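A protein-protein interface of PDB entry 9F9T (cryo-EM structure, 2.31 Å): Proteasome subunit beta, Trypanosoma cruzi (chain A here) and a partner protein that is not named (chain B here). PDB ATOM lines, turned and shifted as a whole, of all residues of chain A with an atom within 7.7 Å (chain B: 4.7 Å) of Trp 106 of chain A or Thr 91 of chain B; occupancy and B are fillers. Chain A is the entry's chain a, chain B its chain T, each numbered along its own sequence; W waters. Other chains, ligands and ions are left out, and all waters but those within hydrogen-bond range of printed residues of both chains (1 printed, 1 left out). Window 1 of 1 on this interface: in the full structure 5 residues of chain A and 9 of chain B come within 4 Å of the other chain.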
ATOM      1  N   MET A  99      -1.786 -23.994  12.814  1.00  0.00           N
ATOM      2  CA  MET A  99      -2.294 -24.955  11.867  1.00  0.00           C
ATOM      3  C   MET A  99      -2.610 -24.341  10.525  1.00  0.00           C
ATOM      4  O   MET A  99      -2.293 -24.955   9.523  1.00  0.00           O
ATOM      5  CB  MET A  99      -3.588 -25.639  12.306  1.00  0.00           C
ATOM      6  CG  MET A  99      -3.435 -26.481  13.559  1.00  0.00           C
ATOM      7  SD  MET A  99      -2.076 -27.702  13.560  1.00  0.00           S
ATOM      8  CE  MET A  99      -0.705 -26.775  14.272  1.00  0.00           C
ATOM      9  N   LEU A 100      -3.191 -23.150  10.488  1.00  0.00           N
ATOM     10  CA  LEU A 100      -3.376 -22.431   9.231  1.00  0.00           C
ATOM     11  C   LEU A 100      -2.065 -22.035   8.558  1.00  0.00           C
ATOM     12  O   LEU A 100      -1.931 -22.090   7.368  1.00  0.00           O
ATOM     13  CB  LEU A 100      -4.194 -21.176   9.528  1.00  0.00           C
ATOM     14  CG  LEU A 100      -5.668 -21.423   9.423  1.00  0.00           C
ATOM     15  CD1 LEU A 100      -6.470 -20.182   9.829  1.00  0.00           C
ATOM     16  CD2 LEU A 100      -5.986 -21.764   7.956  1.00  0.00           C
ATOM     17  N   LYS A 101      -1.152 -21.500   9.295  1.00  0.00           N
ATOM     18  CA  LYS A 101       0.123 -21.160   8.728  1.00  0.00           C
ATOM     19  C   LYS A 101       0.866 -22.321   8.053  1.00  0.00           C
ATOM     20  O   LYS A 101       1.487 -22.066   7.031  1.00  0.00           O
ATOM     21  CB  LYS A 101       0.993 -20.514   9.785  1.00  0.00           C
ATOM     22  CG  LYS A 101       2.398 -20.164   9.355  1.00  0.00           C
ATOM     23  CD  LYS A 101       3.120 -19.728  10.595  1.00  0.00           C
ATOM     24  CE  LYS A 101       4.613 -19.913  10.564  1.00  0.00           C
ATOM     25  NZ  LYS A 101       5.148 -18.947   9.583  1.00  0.00           N
ATOM     26  N   TYR A 102       0.660 -23.566   8.450  1.00  0.00           N
ATOM     27  CA  TYR A 102       1.341 -24.702   7.825  1.00  0.00           C
ATOM     28  C   TYR A 102       0.498 -25.353   6.733  1.00  0.00           C
ATOM     29  O   TYR A 102       1.034 -25.824   5.765  1.00  0.00           O
ATOM     30  CB  TYR A 102       1.760 -25.649   8.963  1.00  0.00           C
ATOM     31  CG  TYR A 102       2.840 -24.967   9.828  1.00  0.00           C
ATOM     32  CD1 TYR A 102       3.966 -24.451   9.236  1.00  0.00           C
ATOM     33  CD2 TYR A 102       2.714 -24.764  11.195  1.00  0.00           C
ATOM     34  CE1 TYR A 102       4.963 -23.837   9.975  1.00  0.00           C
ATOM     35  CE2 TYR A 102       3.678 -24.095  11.958  1.00  0.00           C
ATOM     36  CZ  TYR A 102       4.843 -23.651  11.344  1.00  0.00           C
ATOM     37  OH  TYR A 102       5.901 -23.007  11.942  1.00  0.00           O
ATOM     38  N   ARG A 103      -0.818 -25.402   6.848  1.00  0.00           N
ATOM     39  CA  ARG A 103      -1.596 -25.755   5.694  1.00  0.00           C
ATOM     40  C   ARG A 103      -1.319 -24.798   4.549  1.00  0.00           C
ATOM     41  O   ARG A 103      -1.320 -25.222   3.396  1.00  0.00           O
ATOM     42  CB  ARG A 103      -3.073 -25.736   5.963  1.00  0.00           C
ATOM     43  CG  ARG A 103      -3.521 -26.821   6.930  1.00  0.00           C
ATOM     44  CD  ARG A 103      -3.406 -28.242   6.434  1.00  0.00           C
ATOM     45  NE  ARG A 103      -4.197 -28.333   5.229  1.00  0.00           N
ATOM     46  CZ  ARG A 103      -5.389 -28.913   5.192  1.00  0.00           C
ATOM     47  NH1 ARG A 103      -5.906 -29.240   4.028  1.00  0.00           N
ATOM     48  NH2 ARG A 103      -6.010 -29.235   6.323  1.00  0.00           N
ATOM     49  N   ILE A 104      -1.018 -23.542   4.848  1.00  0.00           N
ATOM     50  CA  ILE A 104      -0.810 -22.570   3.793  1.00  0.00           C
ATOM     51  C   ILE A 104       0.556 -22.747   3.217  1.00  0.00           C
ATOM     52  O   ILE A 104       0.663 -22.663   2.011  1.00  0.00           O
ATOM     53  CB  ILE A 104      -1.059 -21.117   4.200  1.00  0.00           C
ATOM     54  CG1 ILE A 104      -2.522 -20.926   4.484  1.00  0.00           C
ATOM     55  CG2 ILE A 104      -0.546 -20.108   3.230  1.00  0.00           C
ATOM     56  CD1 ILE A 104      -2.800 -19.548   4.909  1.00  0.00           C
ATOM     57  N   GLN A 105       1.519 -23.100   4.034  1.00  0.00           N
ATOM     58  CA  GLN A 105       2.843 -23.403   3.481  1.00  0.00           C
ATOM     59  C   GLN A 105       2.802 -24.671   2.607  1.00  0.00           C
ATOM     60  O   GLN A 105       3.374 -24.720   1.526  1.00  0.00           O
ATOM     61  CB  GLN A 105       3.868 -23.411   4.617  1.00  0.00           C
ATOM     62  CG  GLN A 105       5.264 -23.069   4.120  1.00  0.00           C
ATOM     63  CD  GLN A 105       6.265 -22.532   5.137  1.00  0.00           C
ATOM     64  OE1 GLN A 105       7.174 -21.778   4.765  1.00  0.00           O
ATOM     65  NE2 GLN A 105       6.184 -22.981   6.387  1.00  0.00           N
ATOM     66  N   TRP A 106       1.996 -25.644   3.006  1.00  0.00           N
ATOM     67  CA  TRP A 106       1.872 -26.834   2.214  1.00  0.00           C
ATOM     68  C   TRP A 106       1.173 -26.536   0.895  1.00  0.00           C
ATOM     69  O   TRP A 106       1.510 -27.154  -0.076  1.00  0.00           O
ATOM     70  CB  TRP A 106       1.164 -27.992   2.935  1.00  0.00           C
ATOM     71  CG  TRP A 106       2.074 -28.787   3.810  1.00  0.00           C
ATOM     72  CD1 TRP A 106       2.004 -28.841   5.164  1.00  0.00           C
ATOM     73  CD2 TRP A 106       3.235 -29.540   3.415  1.00  0.00           C
ATOM     74  NE1 TRP A 106       3.029 -29.607   5.644  1.00  0.00           N
ATOM     75  CE2 TRP A 106       3.798 -30.057   4.603  1.00  0.00           C
ATOM     76  CE3 TRP A 106       3.833 -29.842   2.191  1.00  0.00           C
ATOM     77  CZ2 TRP A 106       4.947 -30.838   4.616  1.00  0.00           C
ATOM     78  CZ3 TRP A 106       4.977 -30.609   2.195  1.00  0.00           C
ATOM     79  CH2 TRP A 106       5.542 -31.064   3.397  1.00  0.00           C
ATOM     80  N   TYR A 107       0.158 -25.712   0.885  1.00  0.00           N
ATOM     81  CA  TYR A 107      -0.470 -25.389  -0.373  1.00  0.00           C
ATOM     82  C   TYR A 107       0.574 -24.861  -1.365  1.00  0.00           C
ATOM     83  O   TYR A 107       0.532 -25.251  -2.525  1.00  0.00           O
ATOM     84  CB  TYR A 107      -1.440 -24.259  -0.122  1.00  0.00           C
ATOM     85  CG  TYR A 107      -2.233 -23.839  -1.331  1.00  0.00           C
ATOM     86  CD1 TYR A 107      -1.844 -22.769  -2.098  1.00  0.00           C
ATOM     87  CD2 TYR A 107      -3.500 -24.374  -1.559  1.00  0.00           C
ATOM     88  CE1 TYR A 107      -2.630 -22.315  -3.143  1.00  0.00           C
ATOM     89  CE2 TYR A 107      -4.302 -23.934  -2.590  1.00  0.00           C
ATOM     90  CZ  TYR A 107      -3.837 -22.918  -3.409  1.00  0.00           C
ATOM     91  OH  TYR A 107      -4.622 -22.440  -4.414  1.00  0.00           O
ATOM     92  N   GLN A 108       1.500 -23.999  -0.881  1.00  0.00           N
ATOM     93  CA  GLN A 108       2.402 -23.325  -1.747  1.00  0.00           C
ATOM     94  C   GLN A 108       3.350 -24.335  -2.385  1.00  0.00           C
ATOM     95  O   GLN A 108       3.731 -24.268  -3.576  1.00  0.00           O
ATOM     96  CB  GLN A 108       3.269 -22.340  -1.014  1.00  0.00           C
ATOM     97  CG  GLN A 108       2.703 -20.955  -0.905  1.00  0.00           C
ATOM     98  CD  GLN A 108       3.748 -20.022  -0.315  1.00  0.00           C
ATOM     99  OE1 GLN A 108       4.105 -20.125   0.851  1.00  0.00           O
ATOM    100  NE2 GLN A 108       4.286 -19.121  -1.117  1.00  0.00           N
ATOM    101  N   TYR A 109       3.817 -25.265  -1.553  1.00  0.00           N
ATOM    102  CA  TYR A 109       4.748 -26.271  -2.016  1.00  0.00           C
ATOM    103  C   TYR A 109       4.052 -27.156  -3.017  1.00  0.00           C
ATOM    104  O   TYR A 109       4.705 -27.511  -3.962  1.00  0.00           O
ATOM    105  CB  TYR A 109       5.294 -27.139  -0.888  1.00  0.00           C
ATOM    106  CG  TYR A 109       6.195 -26.429   0.110  1.00  0.00           C
ATOM    107  CD1 TYR A 109       7.090 -25.475  -0.271  1.00  0.00           C
ATOM    108  CD2 TYR A 109       6.198 -26.787   1.445  1.00  0.00           C
ATOM    109  CE1 TYR A 109       8.038 -24.982   0.626  1.00  0.00           C
ATOM    110  CE2 TYR A 109       7.056 -26.221   2.379  1.00  0.00           C
ATOM    111  CZ  TYR A 109       8.010 -25.343   1.951  1.00  0.00           C
ATOM    112  OH  TYR A 109       8.891 -24.823   2.850  1.00  0.00           O
ATOM    113  N   ASN A 110       2.759 -27.441  -2.857  1.00  0.00           N
ATOM    114  CA  ASN A 110       2.047 -28.340  -3.763  1.00  0.00           C
ATOM    115  C   ASN A 110       1.428 -27.614  -4.975  1.00  0.00           C
ATOM    116  O   ASN A 110       0.697 -28.217  -5.757  1.00  0.00           O
ATOM    117  CB  ASN A 110       0.848 -29.037  -3.088  1.00  0.00           C
ATOM    118  CG  ASN A 110       1.201 -29.934  -1.916  1.00  0.00           C
ATOM    119  OD1 ASN A 110       2.263 -30.550  -1.882  1.00  0.00           O
ATOM    120  ND2 ASN A 110       0.314 -30.032  -0.945  1.00  0.00           N
ATOM    121  N   ASN A 111       1.607 -26.288  -5.051  1.00  0.00           N
ATOM    122  CA  ASN A 111       0.907 -25.459  -6.015  1.00  0.00           C
ATOM    123  C   ASN A 111       1.874 -24.515  -6.699  1.00  0.00           C
ATOM    124  O   ASN A 111       1.498 -23.425  -7.098  1.00  0.00           O
ATOM    125  CB  ASN A 111      -0.190 -24.580  -5.441  1.00  0.00           C
ATOM    126  CG  ASN A 111      -1.476 -25.356  -5.227  1.00  0.00           C
ATOM    127  OD1 ASN A 111      -2.441 -25.300  -6.007  1.00  0.00           O
ATOM    128  ND2 ASN A 111      -1.501 -26.119  -4.160  1.00  0.00           N
ATOM    129  N   GLY A 112       3.115 -24.914  -6.841  1.00  0.00           N
ATOM    130  CA  GLY A 112       3.951 -24.127  -7.706  1.00  0.00           C
ATOM    131  C   GLY A 112       4.318 -22.783  -7.102  1.00  0.00           C
ATOM    132  O   GLY A 112       4.736 -21.878  -7.835  1.00  0.00           O
ATOM    133  N   LYS A 114       2.443 -20.674  -5.411  1.00  0.00           N
ATOM    134  CA  LYS A 114       1.369 -19.698  -5.316  1.00  0.00           C
ATOM    135  C   LYS A 114       0.728 -19.727  -3.942  1.00  0.00           C
ATOM    136  O   LYS A 114       0.661 -20.760  -3.301  1.00  0.00           O
ATOM    137  CB  LYS A 114       0.249 -19.991  -6.318  1.00  0.00           C
ATOM    138  CG  LYS A 114       0.363 -19.288  -7.665  1.00  0.00           C
ATOM    139  CD  LYS A 114       1.143 -20.080  -8.657  1.00  0.00           C
ATOM    140  CE  LYS A 114       1.702 -19.215  -9.772  1.00  0.00           C
ATOM    141  NZ  LYS A 114       2.440 -20.026 -10.778  1.00  0.00           N
ATOM    142  N   ARG B  87       9.780 -33.801   1.237  1.00  0.00           N
ATOM    143  CA  ARG B  87       8.630 -33.803   2.153  1.00  0.00           C
ATOM    144  C   ARG B  87       9.189 -33.989   3.558  1.00  0.00           C
ATOM    145  O   ARG B  87       8.712 -33.420   4.543  1.00  0.00           O
ATOM    146  CB  ARG B  87       7.597 -34.847   1.761  1.00  0.00           C
ATOM    147  CG  ARG B  87       6.463 -35.031   2.746  1.00  0.00           C
ATOM    148  CD  ARG B  87       5.361 -35.970   2.242  1.00  0.00           C
ATOM    149  NE  ARG B  87       4.427 -35.326   1.321  1.00  0.00           N
ATOM    150  CZ  ARG B  87       3.563 -34.352   1.653  1.00  0.00           C
ATOM    151  NH1 ARG B  87       2.902 -33.702   0.708  1.00  0.00           N
ATOM    152  NH2 ARG B  87       3.389 -33.989   2.918  1.00  0.00           N
ATOM    153  N   PHE B  88      10.275 -34.756   3.634  1.00  0.00           N
ATOM    154  CA  PHE B  88      10.793 -35.073   4.938  1.00  0.00           C
ATOM    155  C   PHE B  88      11.452 -33.874   5.622  1.00  0.00           C
ATOM    156  O   PHE B  88      11.199 -33.654   6.801  1.00  0.00           O
ATOM    157  CB  PHE B  88      11.764 -36.236   4.847  1.00  0.00           C
ATOM    158  CG  PHE B  88      12.459 -36.506   6.148  1.00  0.00           C
ATOM    159  CD1 PHE B  88      11.778 -37.040   7.190  1.00  0.00           C
ATOM    160  CD2 PHE B  88      13.797 -36.205   6.310  1.00  0.00           C
ATOM    161  CE1 PHE B  88      12.437 -37.357   8.365  1.00  0.00           C
ATOM    162  CE2 PHE B  88      14.465 -36.557   7.458  1.00  0.00           C
ATOM    163  CZ  PHE B  88      13.758 -37.083   8.512  1.00  0.00           C
ATOM    164  N   VAL B  89      12.316 -33.141   4.944  1.00  0.00           N
ATOM    165  CA  VAL B  89      12.974 -32.028   5.579  1.00  0.00           C
ATOM    166  C   VAL B  89      11.978 -30.895   5.895  1.00  0.00           C
ATOM    167  O   VAL B  89      12.132 -30.155   6.858  1.00  0.00           O
ATOM    168  CB  VAL B  89      14.124 -31.546   4.702  1.00  0.00           C
ATOM    169  CG1 VAL B  89      14.835 -30.362   5.329  1.00  0.00           C
ATOM    170  CG2 VAL B  89      15.165 -32.632   4.412  1.00  0.00           C
ATOM    171  N   ARG B  90      10.931 -30.756   5.086  1.00  0.00           N
ATOM    172  CA  ARG B  90      10.036 -29.632   5.177  1.00  0.00           C
ATOM    173  C   ARG B  90       9.249 -29.812   6.446  1.00  0.00           C
ATOM    174  O   ARG B  90       8.850 -28.850   7.125  1.00  0.00           O
ATOM    175  CB  ARG B  90       9.102 -29.567   3.968  1.00  0.00           C
ATOM    176  CG  ARG B  90       9.759 -28.991   2.712  1.00  0.00           C
ATOM    177  CD  ARG B  90       8.916 -29.229   1.442  1.00  0.00           C
ATOM    178  NE  ARG B  90       9.541 -28.487   0.321  1.00  0.00           N
ATOM    179  CZ  ARG B  90       9.127 -28.506  -0.944  1.00  0.00           C
ATOM    180  NH1 ARG B  90       8.220 -29.374  -1.294  1.00  0.00           N
ATOM    181  NH2 ARG B  90       9.627 -27.660  -1.829  1.00  0.00           N
ATOM    182  N   THR B  91       8.965 -31.070   6.710  1.00  0.00           N
ATOM    183  CA  THR B  91       8.134 -31.436   7.840  1.00  0.00           C
ATOM    184  C   THR B  91       8.990 -31.368   9.095  1.00  0.00           C
ATOM    185  O   THR B  91       8.481 -31.016  10.147  1.00  0.00           O
ATOM    186  CB  THR B  91       7.595 -32.844   7.626  1.00  0.00           C
ATOM    187  OG1 THR B  91       6.666 -32.808   6.534  1.00  0.00           O
ATOM    188  CG2 THR B  91       6.979 -33.346   8.898  1.00  0.00           C
ATOM    189  N   GLU B  92      10.289 -31.584   8.969  1.00  0.00           N
ATOM    190  CA  GLU B  92      11.166 -31.386  10.114  1.00  0.00           C
ATOM    191  C   GLU B  92      11.353 -29.912  10.470  1.00  0.00           C
ATOM    192  O   GLU B  92      11.379 -29.602  11.649  1.00  0.00           O
ATOM    193  CB  GLU B  92      12.534 -32.000   9.939  1.00  0.00           C
ATOM    194  CG  GLU B  92      12.415 -33.488  10.094  1.00  0.00           C
ATOM    195  CD  GLU B  92      12.377 -34.031  11.512  1.00  0.00           C
ATOM    196  OE1 GLU B  92      13.350 -33.766  12.305  1.00  0.00           O
ATOM    197  OE2 GLU B  92      11.403 -34.783  11.810  1.00  0.00           O
ATOM    198  N   CYS B  93      11.460 -29.033   9.483  1.00  0.00           N
ATOM    199  CA  CYS B  93      11.686 -27.639   9.764  1.00  0.00           C
ATOM    200  C   CYS B  93      10.449 -26.971  10.322  1.00  0.00           C
ATOM    201  O   CYS B  93      10.541 -26.094  11.180  1.00  0.00           O
ATOM    202  CB  CYS B  93      12.066 -26.931   8.497  1.00  0.00           C
ATOM    203  SG  CYS B  93      13.701 -27.492   7.979  1.00  0.00           S
ATOM    204  N   MET B  94       9.306 -27.345   9.804  1.00  0.00           N
ATOM    205  CA  MET B  94       8.092 -26.812  10.299  1.00  0.00           C
ATOM    206  C   MET B  94       7.945 -27.236  11.750  1.00  0.00           C
ATOM    207  O   MET B  94       7.582 -26.427  12.607  1.00  0.00           O
ATOM    208  CB  MET B  94       6.901 -27.349   9.501  1.00  0.00           C
ATOM    209  CG  MET B  94       6.692 -26.672   8.064  1.00  0.00           C
ATOM    210  SD  MET B  94       5.183 -27.376   7.226  1.00  0.00           S
ATOM    211  CE  MET B  94       5.554 -27.100   5.504  1.00  0.00           C
ATOM    212  N   ASN B  95       8.164 -28.503  12.030  1.00  0.00           N
ATOM    213  CA  ASN B  95       8.014 -28.959  13.374  1.00  0.00           C
ATOM    214  C   ASN B  95       8.891 -28.115  14.270  1.00  0.00           C
ATOM    215  O   ASN B  95       8.428 -27.623  15.321  1.00  0.00           O
ATOM    216  CB  ASN B  95       8.394 -30.420  13.541  1.00  0.00           C
ATOM    217  CG  ASN B  95       7.306 -31.326  13.015  1.00  0.00           C
ATOM    218  OD1 ASN B  95       6.162 -30.888  12.839  1.00  0.00           O
ATOM    219  ND2 ASN B  95       7.687 -32.561  12.678  1.00  0.00           N
HETATM  220  O   HOH W   1       7.855 -27.785  -4.385  1.00  0.00           O
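Met 99 of chain A touches none of the printed residues of chain B.
Of chain B, only Arg 87 (3.7 Å), Arg 90 (3.9 Å), Thr 91 (3.2 Å) and Met 94 (3.5 Å) come within 4 Å of Trp 106 of chain A.
Of the printed residues of chain B, Tyr 109 of chain A touches Arg 90 and Met 94.
Asn 111 of chain A touches none of the printed residues of chain B.
Printed residues of chain A within 4 Å of Arg 90 of chain B: Trp 106 (3.9 Å) and Tyr 109 (3.7 Å).
Thr 91 of chain B touches just one residue of chain A: Trp 106.
The nearest printed residue of chain A that does not touch Arg 90 of chain B is Asn 110 of chain A (6.0 Å).
Among the printed residues, pairs that only touch across the chains: Tyr 102 of chain A with Met 94 of chain B (3.7 Å), Trp 106 of chain A with Arg 87 of chain B (3.7 Å), Trp 106 of chain A with Arg 90 of chain B (3.9 Å), Trp 106 of chain A with Thr 91 of chain B (3.2 Å), Tyr 109 of chain A with Arg 90 of chain B (3.7 Å) and Tyr 109 of chain A with Met 94 of chain B (3.6 Å).
Of the 15 printed residues of chain A, 3 touch a printed residue of chain B.
Printed residues of chain A that touch a printed residue of chain B: Tyr 102, Trp 106 and Tyr 109.
Among the printed residues, no Asp or Glu carboxylate lies within 4 Å of a Lys or Arg side-chain nitrogen of the other chain.
Water W1 bridges NH2 of Arg 90 of chain B and O of Tyr 109 of chain A.
The indole nitrogen (NE1) of Trp 106 of chain A sits at hydrogen-bond distance from the side-chain sulfur (SD) of Met 94 of chain B.
O of Trp 106 of chain A lies within hydrogen-bond range of ND2 of Asn 110 of chain A, at 3.2 Å.
The backbone carbonyl oxygen of Thr 91 of chain B is in hydrogen-bond range of the side-chain amide nitrogen of Asn 95 of chain B, 3.1 Å away.
O of Arg 87 of chain B lies within hydrogen-bond range of OG1 of Thr 91 of chain B, 2.9 Å away.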
